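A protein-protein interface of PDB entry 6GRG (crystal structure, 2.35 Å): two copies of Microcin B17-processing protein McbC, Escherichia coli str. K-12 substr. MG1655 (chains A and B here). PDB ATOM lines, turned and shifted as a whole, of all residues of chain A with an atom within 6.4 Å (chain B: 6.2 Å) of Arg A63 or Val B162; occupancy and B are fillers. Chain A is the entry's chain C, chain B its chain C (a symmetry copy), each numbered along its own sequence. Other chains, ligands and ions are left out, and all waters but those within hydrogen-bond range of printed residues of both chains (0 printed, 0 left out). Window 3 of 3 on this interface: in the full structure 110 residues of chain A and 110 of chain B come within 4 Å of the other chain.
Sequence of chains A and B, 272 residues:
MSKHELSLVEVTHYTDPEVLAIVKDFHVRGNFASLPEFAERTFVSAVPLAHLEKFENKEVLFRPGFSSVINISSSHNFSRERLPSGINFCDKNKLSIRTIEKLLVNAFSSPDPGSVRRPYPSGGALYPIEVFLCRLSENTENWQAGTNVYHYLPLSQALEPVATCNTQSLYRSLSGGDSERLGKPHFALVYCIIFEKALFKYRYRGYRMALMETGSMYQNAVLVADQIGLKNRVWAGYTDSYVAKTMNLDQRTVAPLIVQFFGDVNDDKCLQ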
ATOM      1  N   LEU A  61       1.340  17.180   1.917  1.00  0.00           N
ATOM      2  CA  LEU A  61       2.180  16.017   1.778  1.00  0.00           C
ATOM      3  C   LEU A  61       2.870  15.705   3.109  1.00  0.00           C
ATOM      4  O   LEU A  61       3.150  16.591   3.932  1.00  0.00           O
ATOM      5  CB  LEU A  61       3.213  16.272   0.675  1.00  0.00           C
ATOM      6  CG  LEU A  61       2.694  16.363  -0.763  1.00  0.00           C
ATOM      7  CD1 LEU A  61       3.857  16.390  -1.719  1.00  0.00           C
ATOM      8  CD2 LEU A  61       1.765  15.220  -1.121  1.00  0.00           C
ATOM      9  N   PHE A  62       3.138  14.414   3.303  1.00  0.00           N
ATOM     10  CA  PHE A  62       3.925  13.950   4.420  1.00  0.00           C
ATOM     11  C   PHE A  62       5.411  14.218   4.138  1.00  0.00           C
ATOM     12  O   PHE A  62       6.165  14.471   5.096  1.00  0.00           O
ATOM     13  CB  PHE A  62       3.642  12.477   4.709  1.00  0.00           C
ATOM     14  CG  PHE A  62       4.334  11.943   5.936  1.00  0.00           C
ATOM     15  CD1 PHE A  62       3.765  12.100   7.189  1.00  0.00           C
ATOM     16  CD2 PHE A  62       5.542  11.269   5.831  1.00  0.00           C
ATOM     17  CE1 PHE A  62       4.410  11.617   8.318  1.00  0.00           C
ATOM     18  CE2 PHE A  62       6.182  10.788   6.960  1.00  0.00           C
ATOM     19  CZ  PHE A  62       5.609  10.956   8.199  1.00  0.00           C
ATOM     20  N   ARG A  63       5.812  14.189   2.853  1.00  0.00           N
ATOM     21  CA  ARG A  63       7.198  14.597   2.420  1.00  0.00           C
ATOM     22  C   ARG A  63       7.089  15.703   1.366  1.00  0.00           C
ATOM     23  O   ARG A  63       7.208  15.473   0.159  1.00  0.00           O
ATOM     24  CB  ARG A  63       8.020  13.365   2.005  1.00  0.00           C
ATOM     25  CG  ARG A  63       8.447  12.492   3.184  1.00  0.00           C
ATOM     26  CD  ARG A  63       9.464  11.411   2.849  1.00  0.00           C
ATOM     27  NE  ARG A  63       9.932  10.664   4.018  1.00  0.00           N
ATOM     28  CZ  ARG A  63       9.291   9.628   4.571  1.00  0.00           C
ATOM     29  NH1 ARG A  63       8.168   9.183   4.035  1.00  0.00           N
ATOM     30  NH2 ARG A  63       9.757   9.044   5.664  1.00  0.00           N
ATOM     31  N   PRO A  64       6.808  16.958   1.789  1.00  0.00           N
ATOM     32  CA  PRO A  64       6.572  18.044   0.843  1.00  0.00           C
ATOM     33  C   PRO A  64       7.793  18.196  -0.076  1.00  0.00           C
ATOM     34  O   PRO A  64       8.924  17.913   0.318  1.00  0.00           O
ATOM     35  CB  PRO A  64       6.324  19.283   1.720  1.00  0.00           C
ATOM     36  CG  PRO A  64       5.970  18.736   3.078  1.00  0.00           C
ATOM     37  CD  PRO A  64       6.698  17.413   3.182  1.00  0.00           C
ATOM     38  N   GLY A  65       7.541  18.570  -1.328  1.00  0.00           N
ATOM     39  CA  GLY A  65       8.601  18.727  -2.311  1.00  0.00           C
ATOM     40  C   GLY A  65       9.039  17.427  -2.975  1.00  0.00           C
ATOM     41  O   GLY A  65       9.838  17.486  -3.900  1.00  0.00           O
ATOM     42  N   PHE A  66       8.513  16.276  -2.537  1.00  0.00           N
ATOM     43  CA  PHE A  66       8.852  14.938  -3.106  1.00  0.00           C
ATOM     44  C   PHE A  66       7.603  14.314  -3.744  1.00  0.00           C
ATOM     45  O   PHE A  66       6.499  14.656  -3.417  1.00  0.00           O
ATOM     46  CB  PHE A  66       9.521  14.080  -2.029  1.00  0.00           C
ATOM     47  CG  PHE A  66      10.804  14.705  -1.531  1.00  0.00           C
ATOM     48  CD1 PHE A  66      11.985  14.550  -2.240  1.00  0.00           C
ATOM     49  CD2 PHE A  66      10.807  15.549  -0.433  1.00  0.00           C
ATOM     50  CE1 PHE A  66      13.154  15.163  -1.815  1.00  0.00           C
ATOM     51  CE2 PHE A  66      11.974  16.165  -0.018  1.00  0.00           C
ATOM     52  CZ  PHE A  66      13.143  15.970  -0.707  1.00  0.00           C
ATOM     53  N   SER A  67       7.805  13.411  -4.690  1.00  0.00           N
ATOM     54  CA  SER A  67       6.754  13.002  -5.581  1.00  0.00           C
ATOM     55  C   SER A  67       6.654  11.475  -5.666  1.00  0.00           C
ATOM     56  O   SER A  67       5.818  10.953  -6.388  1.00  0.00           O
ATOM     57  CB  SER A  67       7.006  13.588  -6.942  1.00  0.00           C
ATOM     58  OG  SER A  67       8.196  13.065  -7.510  1.00  0.00           O
ATOM     59  N   GLU B   5      -0.564  20.120  -4.700  1.00  0.00           N
ATOM     60  CA  GLU B   5       0.155  20.215  -3.456  1.00  0.00           C
ATOM     61  C   GLU B   5      -0.132  21.562  -2.783  1.00  0.00           C
ATOM     62  O   GLU B   5      -0.170  22.584  -3.433  1.00  0.00           O
ATOM     63  CB  GLU B   5       1.660  20.066  -3.703  1.00  0.00           C
ATOM     64  CG  GLU B   5       2.470  19.952  -2.424  1.00  0.00           C
ATOM     65  CD  GLU B   5       3.934  19.607  -2.598  1.00  0.00           C
ATOM     66  OE1 GLU B   5       4.373  19.463  -3.753  1.00  0.00           O
ATOM     67  OE2 GLU B   5       4.624  19.476  -1.567  1.00  0.00           O
ATOM     68  N   PHE B 132      -4.498   8.108   6.991  1.00  0.00           N
ATOM     69  CA  PHE B 132      -3.309   7.274   7.020  1.00  0.00           C
ATOM     70  C   PHE B 132      -3.747   5.813   7.036  1.00  0.00           C
ATOM     71  O   PHE B 132      -4.803   5.493   7.554  1.00  0.00           O
ATOM     72  CB  PHE B 132      -2.418   7.635   8.208  1.00  0.00           C
ATOM     73  CG  PHE B 132      -1.662   8.936   8.072  1.00  0.00           C
ATOM     74  CD1 PHE B 132      -2.237  10.134   8.459  1.00  0.00           C
ATOM     75  CD2 PHE B 132      -0.371   8.964   7.553  1.00  0.00           C
ATOM     76  CE1 PHE B 132      -1.541  11.330   8.342  1.00  0.00           C
ATOM     77  CE2 PHE B 132       0.321  10.160   7.435  1.00  0.00           C
ATOM     78  CZ  PHE B 132      -0.267  11.341   7.825  1.00  0.00           C
ATOM     79  N   THR B 147       7.152  -1.349   4.579  1.00  0.00           N
ATOM     80  CA  THR B 147       6.376  -0.109   4.867  1.00  0.00           C
ATOM     81  C   THR B 147       4.960  -0.477   5.317  1.00  0.00           C
ATOM     82  O   THR B 147       4.217  -1.044   4.549  1.00  0.00           O
ATOM     83  CB  THR B 147       6.331   0.846   3.668  1.00  0.00           C
ATOM     84  OG1 THR B 147       7.684   1.199   3.416  1.00  0.00           O
ATOM     85  CG2 THR B 147       5.533   2.106   3.912  1.00  0.00           C
ATOM     86  N   VAL B 149       3.043   1.978   7.359  1.00  0.00           N
ATOM     87  CA  VAL B 149       2.215   3.168   7.407  1.00  0.00           C
ATOM     88  C   VAL B 149       2.326   3.877   6.064  1.00  0.00           C
ATOM     89  O   VAL B 149       3.388   4.008   5.519  1.00  0.00           O
ATOM     90  CB  VAL B 149       2.567   4.101   8.575  1.00  0.00           C
ATOM     91  CG1 VAL B 149       1.483   5.144   8.762  1.00  0.00           C
ATOM     92  CG2 VAL B 149       2.784   3.329   9.867  1.00  0.00           C
ATOM     93  N   TYR B 150       1.181   4.301   5.545  1.00  0.00           N
ATOM     94  CA  TYR B 150       1.095   5.050   4.325  1.00  0.00           C
ATOM     95  C   TYR B 150       0.155   6.234   4.580  1.00  0.00           C
ATOM     96  O   TYR B 150      -0.646   6.203   5.526  1.00  0.00           O
ATOM     97  CB  TYR B 150       0.583   4.183   3.160  1.00  0.00           C
ATOM     98  CG  TYR B 150       1.431   3.001   2.745  1.00  0.00           C
ATOM     99  CD1 TYR B 150       1.231   1.740   3.298  1.00  0.00           C
ATOM    100  CD2 TYR B 150       2.394   3.121   1.751  1.00  0.00           C
ATOM    101  CE1 TYR B 150       1.993   0.649   2.912  1.00  0.00           C
ATOM    102  CE2 TYR B 150       3.167   2.037   1.354  1.00  0.00           C
ATOM    103  CZ  TYR B 150       2.962   0.793   1.930  1.00  0.00           C
ATOM    104  OH  TYR B 150       3.705  -0.281   1.525  1.00  0.00           O
ATOM    105  N   HIS B 151       0.284   7.269   3.740  1.00  0.00           N
ATOM    106  CA  HIS B 151      -0.605   8.435   3.710  1.00  0.00           C
ATOM    107  C   HIS B 151      -1.370   8.406   2.383  1.00  0.00           C
ATOM    108  O   HIS B 151      -0.741   8.307   1.348  1.00  0.00           O
ATOM    109  CB  HIS B 151       0.223   9.713   3.915  1.00  0.00           C
ATOM    110  CG  HIS B 151      -0.537  10.979   3.739  1.00  0.00           C
ATOM    111  ND1 HIS B 151       0.070  12.140   3.298  1.00  0.00           N
ATOM    112  CD2 HIS B 151      -1.843  11.281   3.926  1.00  0.00           C
ATOM    113  CE1 HIS B 151      -0.820  13.108   3.247  1.00  0.00           C
ATOM    114  NE2 HIS B 151      -2.004  12.612   3.625  1.00  0.00           N
ATOM    115  N   GLU B 160       1.551   7.498  -0.111  1.00  0.00           N
ATOM    116  CA  GLU B 160       2.836   8.072   0.252  1.00  0.00           C
ATOM    117  C   GLU B 160       3.362   7.266   1.436  1.00  0.00           C
ATOM    118  O   GLU B 160       2.678   7.189   2.438  1.00  0.00           O
ATOM    119  CB  GLU B 160       2.580   9.558   0.530  1.00  0.00           C
ATOM    120  CG  GLU B 160       3.799  10.413   0.820  1.00  0.00           C
ATOM    121  CD  GLU B 160       3.442  11.865   1.116  1.00  0.00           C
ATOM    122  OE1 GLU B 160       2.261  12.138   1.374  1.00  0.00           O
ATOM    123  OE2 GLU B 160       4.340  12.725   1.087  1.00  0.00           O
ATOM    124  N   PRO B 161       4.507   6.547   1.324  1.00  0.00           N
ATOM    125  CA  PRO B 161       5.143   5.880   2.465  1.00  0.00           C
ATOM    126  C   PRO B 161       5.334   6.805   3.668  1.00  0.00           C
ATOM    127  O   PRO B 161       5.713   7.947   3.489  1.00  0.00           O
ATOM    128  CB  PRO B 161       6.558   5.531   1.972  1.00  0.00           C
ATOM    129  CG  PRO B 161       6.430   5.433   0.470  1.00  0.00           C
ATOM    130  CD  PRO B 161       5.231   6.272   0.071  1.00  0.00           C
ATOM    131  N   VAL B 162       5.115   6.288   4.879  1.00  0.00           N
ATOM    132  CA  VAL B 162       5.204   7.109   6.066  1.00  0.00           C
ATOM    133  C   VAL B 162       6.201   6.488   7.052  1.00  0.00           C
ATOM    134  O   VAL B 162       7.041   7.200   7.587  1.00  0.00           O
ATOM    135  CB  VAL B 162       3.798   7.324   6.663  1.00  0.00           C
ATOM    136  CG1 VAL B 162       3.833   7.997   8.024  1.00  0.00           C
ATOM    137  CG2 VAL B 162       2.936   8.115   5.698  1.00  0.00           C
ATOM    138  N   ALA B 163       6.100   5.177   7.304  1.00  0.00           N
ATOM    139  CA  ALA B 163       6.829   4.543   8.400  1.00  0.00           C
ATOM    140  C   ALA B 163       7.060   3.055   8.127  1.00  0.00           C
ATOM    141  O   ALA B 163       6.204   2.344   7.560  1.00  0.00           O
ATOM    142  CB  ALA B 163       6.082   4.731   9.702  1.00  0.00           C
ATOM    143  N   THR B 164       8.216   2.586   8.599  1.00  0.00           N
ATOM    144  CA  THR B 164       8.566   1.202   8.501  1.00  0.00           C
ATOM    145  C   THR B 164       8.553   0.559   9.896  1.00  0.00           C
ATOM    146  O   THR B 164       9.227  -0.429  10.115  1.00  0.00           O
ATOM    147  CB  THR B 164       9.931   1.020   7.824  1.00  0.00           C
ATOM    148  OG1 THR B 164      10.903   1.484   8.764  1.00  0.00           O
ATOM    149  CG2 THR B 164      10.056   1.761   6.509  1.00  0.00           C
ATOM    150  N   MET B 247       3.465   6.400  14.028  1.00  0.00           N
ATOM    151  CA  MET B 247       3.234   6.797  12.658  1.00  0.00           C
ATOM    152  C   MET B 247       4.167   7.944  12.222  1.00  0.00           C
ATOM    153  O   MET B 247       4.081   8.398  11.102  1.00  0.00           O
ATOM    154  CB  MET B 247       1.782   7.255  12.541  1.00  0.00           C
ATOM    155  CG  MET B 247       0.812   6.091  12.531  1.00  0.00           C
ATOM    156  SD  MET B 247      -0.867   6.720  12.565  1.00  0.00           S
ATOM    157  CE  MET B 247      -1.072   7.177  10.848  1.00  0.00           C
ATOM    158  N   ASN B 248       5.011   8.428  13.143  1.00  0.00           N
ATOM    159  CA  ASN B 248       5.993   9.492  12.929  1.00  0.00           C
ATOM    160  C   ASN B 248       5.298  10.821  12.566  1.00  0.00           C
ATOM    161  O   ASN B 248       5.863  11.657  11.898  1.00  0.00           O
ATOM    162  CB  ASN B 248       7.071   9.045  11.930  1.00  0.00           C
ATOM    163  CG  ASN B 248       8.084   8.070  12.508  1.00  0.00           C
ATOM    164  OD1 ASN B 248       8.608   8.263  13.598  1.00  0.00           O
ATOM    165  ND2 ASN B 248       8.401   7.028  11.766  1.00  0.00           N
ATOM    166  N   LEU B 249       4.083  11.032  13.061  1.00  0.00           N
ATOM    167  CA  LEU B 249       3.417  12.334  13.004  1.00  0.00           C
ATOM    168  C   LEU B 249       4.023  13.255  14.074  1.00  0.00           C
ATOM    169  O   LEU B 249       4.390  12.821  15.136  1.00  0.00           O
ATOM    170  CB  LEU B 249       1.913  12.177  13.250  1.00  0.00           C
ATOM    171  CG  LEU B 249       1.168  11.144  12.399  1.00  0.00           C
ATOM    172  CD1 LEU B 249      -0.297  11.090  12.810  1.00  0.00           C
ATOM    173  CD2 LEU B 249       1.274  11.431  10.911  1.00  0.00           C
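The backbone NH (N) of Phe A62 lies within hydrogen-bond range of the side-chain carboxylate (OE2) of Glu B160 (3.0 Å).
N of Arg A63 sits at hydrogen-bond distance from OE2 of Glu B160, 2.7 Å away.
The guanidinium group (NH1) of Arg A63 sits at hydrogen-bond distance from the backbone carbonyl oxygen (O) of Pro B161, 2.8 Å away.
The backbone NH (N) of Gly A65 sits at hydrogen-bond distance from the side-chain carboxylate (OE2) of Glu B5.
The backbone NH of His B151 is in hydrogen-bond range of the backbone carbonyl oxygen of Glu B160, at 2.7 Å.
The backbone NH (N) of Val B162 sits at hydrogen-bond distance from the backbone carbonyl oxygen (O) of Val B149 (2.9 Å).
CD1 of Leu A61 touches OE2 of Glu B5, at 3.2 Å.
Leu A61 touches Glu B160.
CD1 of Phe A62 touches CE2 of Phe B132, 3.96 Å away.
Phe A62 touches His B151.
CZ of Phe A62 touches CG1 of Val B162, at 3.5 Å.
CZ of Phe A62 touches O of Asn B248, 3.8 Å away.
Arg A63 touches Val B162 (NH2 to O, 3.8 Å).
OE2 of Glu B5 touches CA of Pro A64, 3.4 Å away.
Of the printed residues of chain B, Pro A64 touches Glu B5 (3.4 Å).
Printed residues of chain B within 4 Å of Gly A65: Glu B5 (3.1 Å).
Ser A67 touches none of the printed residues of chain B.
Printed residues of chain A within 4 Å of Phe B132: Phe A62.
Val B149 touches none of the printed residues of chain A.
Printed residues of chain A within 4 Å of His B151: Phe A62.
Of the printed residues of chain A, Glu B160 touches Leu A61, Phe A62 and Arg A63.
Val B162 touches two residues of chain A.
Of the 14 printed residues of chain B, 7 touch a printed residue of chain A.
Hydrophobic or aromatic side chains of chain B that line the printed part of chain A: Phe B132, His B151 and Val B162.
Of the 7 printed residues of chain A, 5 touch a printed residue of chain B.
Hydrophobic or aromatic side chains of chain A within 4 Å of the printed part of chain B: Leu A61, Phe A62 and Pro A64.
Among the printed residues, 12 pairs touch across the chains.
No position is printed for both chains.
Of the 12 pairs that touch across the chains among the printed residues, none has its exchanged pair printed and touching as well.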
